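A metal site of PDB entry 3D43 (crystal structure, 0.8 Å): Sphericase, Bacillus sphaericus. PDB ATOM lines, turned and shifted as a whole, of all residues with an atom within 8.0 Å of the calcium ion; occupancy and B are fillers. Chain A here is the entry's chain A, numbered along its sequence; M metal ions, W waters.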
ATOM      1  N   THR A 200     -22.111 -18.778 -25.011  1.00  0.00           N
ATOM      2  CA  THR A 200     -20.828 -19.282 -25.290  1.00  0.00           C
ATOM      3  C   THR A 200     -20.579 -19.330 -26.781  1.00  0.00           C
ATOM      4  O   THR A 200     -21.513 -19.202 -27.572  1.00  0.00           O
ATOM      5  CB  THR A 200     -20.570 -20.698 -24.694  1.00  0.00           C
ATOM      6  OG1 THR A 200     -21.185 -21.707 -25.508  1.00  0.00           O
ATOM      7  CG2 THR A 200     -21.103 -20.842 -23.298  1.00  0.00           C
ATOM      8  N   VAL A 203     -20.595 -24.561 -31.321  1.00  0.00           N
ATOM      9  CA  VAL A 203     -19.995 -25.591 -32.138  1.00  0.00           C
ATOM     10  C   VAL A 203     -20.581 -25.514 -33.547  1.00  0.00           C
ATOM     11  O   VAL A 203     -21.800 -25.380 -33.734  1.00  0.00           O
ATOM     12  CB  VAL A 203     -20.292 -26.982 -31.553  1.00  0.00           C
ATOM     13  CG1 VAL A 203     -19.657 -28.083 -32.415  1.00  0.00           C
ATOM     14  CG2 VAL A 203     -19.807 -27.086 -30.110  1.00  0.00           C
ATOM     15  N   TYR A 218     -16.283 -36.148 -17.767  1.00  0.00           N
ATOM     16  CA  TYR A 218     -14.952 -35.517 -17.811  1.00  0.00           C
ATOM     17  C   TYR A 218     -13.843 -36.552 -17.725  1.00  0.00           C
ATOM     18  O   TYR A 218     -12.773 -36.250 -17.169  1.00  0.00           O
ATOM     19  CB  TYR A 218     -14.846 -34.414 -16.759  1.00  0.00           C
ATOM     20  CG  TYR A 218     -15.614 -33.150 -16.973  1.00  0.00           C
ATOM     21  CD1 TYR A 218     -16.783 -32.963 -16.235  1.00  0.00           C
ATOM     22  CD2 TYR A 218     -15.234 -32.196 -17.876  1.00  0.00           C
ATOM     23  CE1 TYR A 218     -17.534 -31.811 -16.407  1.00  0.00           C
ATOM     24  CE2 TYR A 218     -15.970 -31.020 -18.023  1.00  0.00           C
ATOM     25  CZ  TYR A 218     -17.125 -30.829 -17.302  1.00  0.00           C
ATOM     26  OH  TYR A 218     -17.843 -29.672 -17.423  1.00  0.00           O
ATOM     27  N   SER A 228     -12.745 -28.127 -27.631  1.00  0.00           N
ATOM     28  CA  SER A 228     -13.220 -27.326 -28.744  1.00  0.00           C
ATOM     29  C   SER A 228     -12.273 -26.159 -29.031  1.00  0.00           C
ATOM     30  O   SER A 228     -11.669 -25.614 -28.100  1.00  0.00           O
ATOM     31  CB  SER A 228     -14.590 -26.785 -28.407  1.00  0.00           C
ATOM     32  OG  SER A 228     -15.567 -27.797 -28.268  1.00  0.00           O
ATOM     33  N   ALA A 283      -9.976 -26.538 -20.546  1.00  0.00           N
ATOM     34  CA  ALA A 283     -11.252 -26.646 -21.263  1.00  0.00           C
ATOM     35  C   ALA A 283     -12.409 -26.694 -20.343  1.00  0.00           C
ATOM     36  O   ALA A 283     -13.430 -26.051 -20.578  1.00  0.00           O
ATOM     37  CB  ALA A 283     -11.204 -27.906 -22.145  1.00  0.00           C
ATOM     38  N   LYS A 284     -12.343 -27.472 -19.272  1.00  0.00           N
ATOM     39  CA  LYS A 284     -13.445 -27.629 -18.371  1.00  0.00           C
ATOM     40  C   LYS A 284     -13.883 -26.275 -17.794  1.00  0.00           C
ATOM     41  O   LYS A 284     -15.075 -26.056 -17.540  1.00  0.00           O
ATOM     42  CB  LYS A 284     -13.069 -28.591 -17.228  1.00  0.00           C
ATOM     43  CG  LYS A 284     -14.123 -28.735 -16.162  1.00  0.00           C
ATOM     44  CD  LYS A 284     -13.674 -29.824 -15.186  1.00  0.00           C
ATOM     45  CE  LYS A 284     -14.701 -30.205 -14.185  1.00  0.00           C
ATOM     46  NZ  LYS A 284     -14.115 -31.198 -13.197  1.00  0.00           N
ATOM     47  N   VAL A 286     -14.083 -23.492 -19.274  1.00  0.00           N
ATOM     48  CA  VAL A 286     -14.792 -22.705 -20.285  1.00  0.00           C
ATOM     49  C   VAL A 286     -15.791 -23.643 -20.980  1.00  0.00           C
ATOM     50  O   VAL A 286     -15.591 -24.182 -22.031  1.00  0.00           O
ATOM     51  CB  VAL A 286     -13.853 -22.055 -21.316  1.00  0.00           C
ATOM     52  CG1 VAL A 286     -14.653 -21.153 -22.207  1.00  0.00           C
ATOM     53  CG2 VAL A 286     -12.756 -21.303 -20.545  1.00  0.00           C
ATOM     54  N   ASP A 287     -16.928 -23.818 -20.270  1.00  0.00           N
ATOM     55  CA  ASP A 287     -17.961 -24.724 -20.767  1.00  0.00           C
ATOM     56  C   ASP A 287     -18.595 -24.193 -22.025  1.00  0.00           C
ATOM     57  O   ASP A 287     -19.347 -23.191 -21.938  1.00  0.00           O
ATOM     58  CB  ASP A 287     -18.992 -24.875 -19.656  1.00  0.00           C
ATOM     59  CG  ASP A 287     -20.066 -25.901 -19.867  1.00  0.00           C
ATOM     60  OD1 ASP A 287     -20.001 -26.568 -20.918  1.00  0.00           O
ATOM     61  OD2 ASP A 287     -20.933 -26.018 -18.971  1.00  0.00           O
ATOM     62  N   ILE A 288     -18.631 -24.989 -23.081  1.00  0.00           N
ATOM     63  CA  ILE A 288     -19.325 -24.651 -24.315  1.00  0.00           C
ATOM     64  C   ILE A 288     -20.765 -25.188 -24.229  1.00  0.00           C
ATOM     65  O   ILE A 288     -20.971 -26.376 -23.891  1.00  0.00           O
ATOM     66  CB  ILE A 288     -18.591 -25.169 -25.523  1.00  0.00           C
ATOM     67  CG1 ILE A 288     -17.247 -24.457 -25.664  1.00  0.00           C
ATOM     68  CG2 ILE A 288     -19.404 -25.087 -26.779  1.00  0.00           C
ATOM     69  CD1 ILE A 288     -17.361 -22.980 -25.977  1.00  0.00           C
ATOM     70  N   LYS A 289     -21.721 -24.357 -24.578  1.00  0.00           N
ATOM     71  CA  LYS A 289     -23.143 -24.715 -24.466  1.00  0.00           C
ATOM     72  C   LYS A 289     -23.908 -24.433 -25.742  1.00  0.00           C
ATOM     73  O   LYS A 289     -25.139 -24.644 -25.742  1.00  0.00           O
ATOM     74  CB  LYS A 289     -23.720 -23.968 -23.294  1.00  0.00           C
ATOM     75  CG  LYS A 289     -22.989 -24.250 -21.993  1.00  0.00           C
ATOM     76  CD  LYS A 289     -23.717 -23.689 -20.768  1.00  0.00           C
ATOM     77  CE  LYS A 289     -23.150 -22.373 -20.298  1.00  0.00           C
ATOM     78  NZ  LYS A 289     -24.077 -21.769 -19.262  1.00  0.00           N
ATOM     79  N   GLY A 290     -23.253 -23.989 -26.803  1.00  0.00           N
ATOM     80  CA  GLY A 290     -23.962 -23.663 -28.052  1.00  0.00           C
ATOM     81  C   GLY A 290     -23.687 -24.700 -29.120  1.00  0.00           C
ATOM     82  O   GLY A 290     -22.538 -25.186 -29.233  1.00  0.00           O
ATOM     83  N   GLY A 293     -26.442 -30.616 -29.553  1.00  0.00           N
ATOM     84  CA  GLY A 293     -25.878 -31.550 -28.603  1.00  0.00           C
ATOM     85  C   GLY A 293     -25.087 -30.886 -27.486  1.00  0.00           C
ATOM     86  O   GLY A 293     -24.769 -31.565 -26.496  1.00  0.00           O
ATOM     87  N   ALA A 294     -24.751 -29.604 -27.623  1.00  0.00           N
ATOM     88  CA  ALA A 294     -24.039 -28.946 -26.559  1.00  0.00           C
ATOM     89  C   ALA A 294     -24.881 -28.756 -25.342  1.00  0.00           C
ATOM     90  O   ALA A 294     -26.092 -28.491 -25.430  1.00  0.00           O
ATOM     91  CB  ALA A 294     -23.448 -27.620 -27.061  1.00  0.00           C
ATOM     92  N   ALA A 295     -24.267 -28.832 -24.174  1.00  0.00           N
ATOM     93  CA  ALA A 295     -25.019 -28.849 -22.886  1.00  0.00           C
ATOM     94  C   ALA A 295     -24.168 -28.271 -21.813  1.00  0.00           C
ATOM     95  O   ALA A 295     -22.919 -28.091 -21.918  1.00  0.00           O
ATOM     96  CB  ALA A 295     -25.315 -30.317 -22.571  1.00  0.00           C
ATOM     97  N   ILE A 296     -24.732 -27.974 -20.667  1.00  0.00           N
ATOM     98  CA  ILE A 296     -23.990 -27.710 -19.454  1.00  0.00           C
ATOM     99  C   ILE A 296     -23.078 -28.919 -19.185  1.00  0.00           C
ATOM    100  O   ILE A 296     -23.531 -30.066 -19.222  1.00  0.00           O
ATOM    101  CB  ILE A 296     -24.932 -27.437 -18.306  1.00  0.00           C
ATOM    102  CG1 ILE A 296     -25.870 -26.233 -18.585  1.00  0.00           C
ATOM    103  CG2 ILE A 296     -24.189 -27.301 -17.020  1.00  0.00           C
ATOM    104  CD1 ILE A 296     -26.995 -26.010 -17.574  1.00  0.00           C
ATOM    105  N   GLY A 297     -21.829 -28.637 -18.924  1.00  0.00           N
ATOM    106  CA  GLY A 297     -20.865 -29.682 -18.588  1.00  0.00           C
ATOM    107  C   GLY A 297     -20.238 -30.320 -19.809  1.00  0.00           C
ATOM    108  O   GLY A 297     -20.255 -29.815 -20.942  1.00  0.00           O
ATOM    109  N   ASP A 298     -19.604 -31.473 -19.597  1.00  0.00           N
ATOM    110  CA  ASP A 298     -18.945 -32.227 -20.640  1.00  0.00           C
ATOM    111  C   ASP A 298     -20.028 -32.802 -21.547  1.00  0.00           C
ATOM    112  O   ASP A 298     -20.930 -33.472 -21.077  1.00  0.00           O
ATOM    113  CB  ASP A 298     -18.128 -33.370 -19.963  1.00  0.00           C
ATOM    114  CG  ASP A 298     -17.552 -34.392 -20.857  1.00  0.00           C
ATOM    115  OD1 ASP A 298     -17.380 -35.555 -20.368  1.00  0.00           O
ATOM    116  OD2 ASP A 298     -17.274 -34.078 -22.031  1.00  0.00           O
ATOM    117  N   ASP A 299     -19.882 -32.555 -22.857  1.00  0.00           N
ATOM    118  CA  ASP A 299     -20.929 -33.018 -23.764  1.00  0.00           C
ATOM    119  C   ASP A 299     -20.346 -33.518 -25.071  1.00  0.00           C
ATOM    120  O   ASP A 299     -19.157 -33.354 -25.345  1.00  0.00           O
ATOM    121  CB  ASP A 299     -21.961 -31.892 -23.998  1.00  0.00           C
ATOM    122  CG  ASP A 299     -21.398 -30.686 -24.688  1.00  0.00           C
ATOM    123  OD1 ASP A 299     -21.359 -29.593 -24.119  1.00  0.00           O
ATOM    124  OD2 ASP A 299     -20.953 -30.845 -25.888  1.00  0.00           O
ATOM    125  N   TYR A 300     -21.166 -34.186 -25.880  1.00  0.00           N
ATOM    126  CA  TYR A 300     -20.687 -34.896 -27.044  1.00  0.00           C
ATOM    127  C   TYR A 300     -20.532 -33.970 -28.263  1.00  0.00           C
ATOM    128  O   TYR A 300     -20.045 -34.436 -29.334  1.00  0.00           O
ATOM    129  CB  TYR A 300     -21.434 -36.170 -27.438  1.00  0.00           C
ATOM    130  CG  TYR A 300     -22.898 -35.857 -27.681  1.00  0.00           C
ATOM    131  CD1 TYR A 300     -23.362 -35.460 -28.920  1.00  0.00           C
ATOM    132  CD2 TYR A 300     -23.753 -35.929 -26.630  1.00  0.00           C
ATOM    133  CE1 TYR A 300     -24.672 -35.161 -29.131  1.00  0.00           C
ATOM    134  CE2 TYR A 300     -25.086 -35.638 -26.798  1.00  0.00           C
ATOM    135  CZ  TYR A 300     -25.539 -35.248 -28.041  1.00  0.00           C
ATOM    136  OH  TYR A 300     -26.842 -34.966 -28.298  1.00  0.00           O
ATOM    137  N   ALA A 301     -20.876 -32.700 -28.159  1.00  0.00           N
ATOM    138  CA  ALA A 301     -20.614 -31.734 -29.241  1.00  0.00           C
ATOM    139  C   ALA A 301     -19.287 -31.023 -29.068  1.00  0.00           C
ATOM    140  O   ALA A 301     -18.564 -30.763 -30.040  1.00  0.00           O
ATOM    141  CB  ALA A 301     -21.706 -30.694 -29.335  1.00  0.00           C
ATOM    142  N   SER A 302     -18.945 -30.646 -27.818  1.00  0.00           N
ATOM    143  CA  SER A 302     -17.844 -29.762 -27.535  1.00  0.00           C
ATOM    144  C   SER A 302     -16.848 -30.360 -26.572  1.00  0.00           C
ATOM    145  O   SER A 302     -15.822 -29.734 -26.265  1.00  0.00           O
ATOM    146  CB  SER A 302     -18.395 -28.445 -27.006  1.00  0.00           C
ATOM    147  OG  SER A 302     -19.061 -28.593 -25.760  1.00  0.00           O
ATOM    148  N   GLY A 303     -17.095 -31.568 -26.062  1.00  0.00           N
ATOM    149  CA  GLY A 303     -16.197 -32.160 -25.089  1.00  0.00           C
ATOM    150  C   GLY A 303     -16.208 -31.380 -23.794  1.00  0.00           C
ATOM    151  O   GLY A 303     -17.278 -30.918 -23.267  1.00  0.00           O
ATOM    152  N   PHE A 304     -15.061 -31.246 -23.197  1.00  0.00           N
ATOM    153  CA  PHE A 304     -14.918 -30.653 -21.904  1.00  0.00           C
ATOM    154  C   PHE A 304     -15.148 -29.137 -21.972  1.00  0.00           C
ATOM    155  O   PHE A 304     -15.521 -28.568 -20.934  1.00  0.00           O
ATOM    156  CB  PHE A 304     -13.517 -30.918 -21.341  1.00  0.00           C
ATOM    157  CG  PHE A 304     -13.240 -32.349 -20.938  1.00  0.00           C
ATOM    158  CD1 PHE A 304     -14.018 -33.444 -21.339  1.00  0.00           C
ATOM    159  CD2 PHE A 304     -12.127 -32.616 -20.163  1.00  0.00           C
ATOM    160  CE1 PHE A 304     -13.655 -34.724 -21.003  1.00  0.00           C
ATOM    161  CE2 PHE A 304     -11.770 -33.881 -19.781  1.00  0.00           C
ATOM    162  CZ  PHE A 304     -12.529 -34.946 -20.247  1.00  0.00           C
ATOM    163  N   GLY A 305     -14.899 -28.533 -23.105  1.00  0.00           N
ATOM    164  CA  GLY A 305     -15.011 -27.095 -23.264  1.00  0.00           C
ATOM    165  C   GLY A 305     -13.928 -26.521 -24.147  1.00  0.00           C
ATOM    166  O   GLY A 305     -13.345 -27.255 -24.972  1.00  0.00           O
ATOM    167  N   PHE A 306     -13.703 -25.220 -24.018  1.00  0.00           N
ATOM    168  CA  PHE A 306     -12.787 -24.462 -24.882  1.00  0.00           C
ATOM    169  C   PHE A 306     -11.544 -24.078 -24.067  1.00  0.00           C
ATOM    170  O   PHE A 306     -11.606 -23.148 -23.270  1.00  0.00           O
ATOM    171  CB  PHE A 306     -13.533 -23.237 -25.398  1.00  0.00           C
ATOM    172  CG  PHE A 306     -12.784 -22.244 -26.235  1.00  0.00           C
ATOM    173  CD1 PHE A 306     -13.264 -20.962 -26.378  1.00  0.00           C
ATOM    174  CD2 PHE A 306     -11.637 -22.574 -26.911  1.00  0.00           C
ATOM    175  CE1 PHE A 306     -12.625 -20.051 -27.184  1.00  0.00           C
ATOM    176  CE2 PHE A 306     -10.959 -21.673 -27.712  1.00  0.00           C
ATOM    177  CZ  PHE A 306     -11.455 -20.387 -27.837  1.00  0.00           C
HETATM  178 CA    CA M   1     -20.699 -28.138 -22.420  1.00  0.00          CA
HETATM  179  O   HOH W   1     -18.470 -28.291 -23.172  1.00  0.00           O
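Residues that only touch the calcium ion: Ser 302.
Within 4 Å of the calcium ion: Asp 287, Ile 288, Ala 295, Gly 297, Asp 299 and Ser 302.
Along chain A the residues within 4 Å of the calcium ion span positions 287 to 302.
Water W1 lies within hydrogen-bond range of the side-chain hydroxyl (OG) of Ser 302 (2.7 Å), the backbone carbonyl oxygen (O) of Gly 303 (2.9 Å) and the backbone NH (N) of Ile 288 (3.3 Å).
O of Ile 288 lies close to OG of Ser 302 (3.5 Å).
OD2 of Asp 299 sits at hydrogen-bond distance from N of Ser 302, 2.8 Å away.
O of Ser 302 is in hydrogen-bond range of OG of Ser 228 (2.8 Å).
OD2 of Asp 299 is in hydrogen-bond range of N of Ala 301, 2.9 Å away.
The calcium ion is bound by O of Ala 295 (2.3 Å), O of Gly 297 (2.3 Å), OD1 of Asp 287 (2.3 Å), O of Ile 288 (2.3 Å), OD1 of Asp 299 (2.3 Å) and water W1 (2.4 Å).
The calcium ion has six donor atoms within binding distance.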
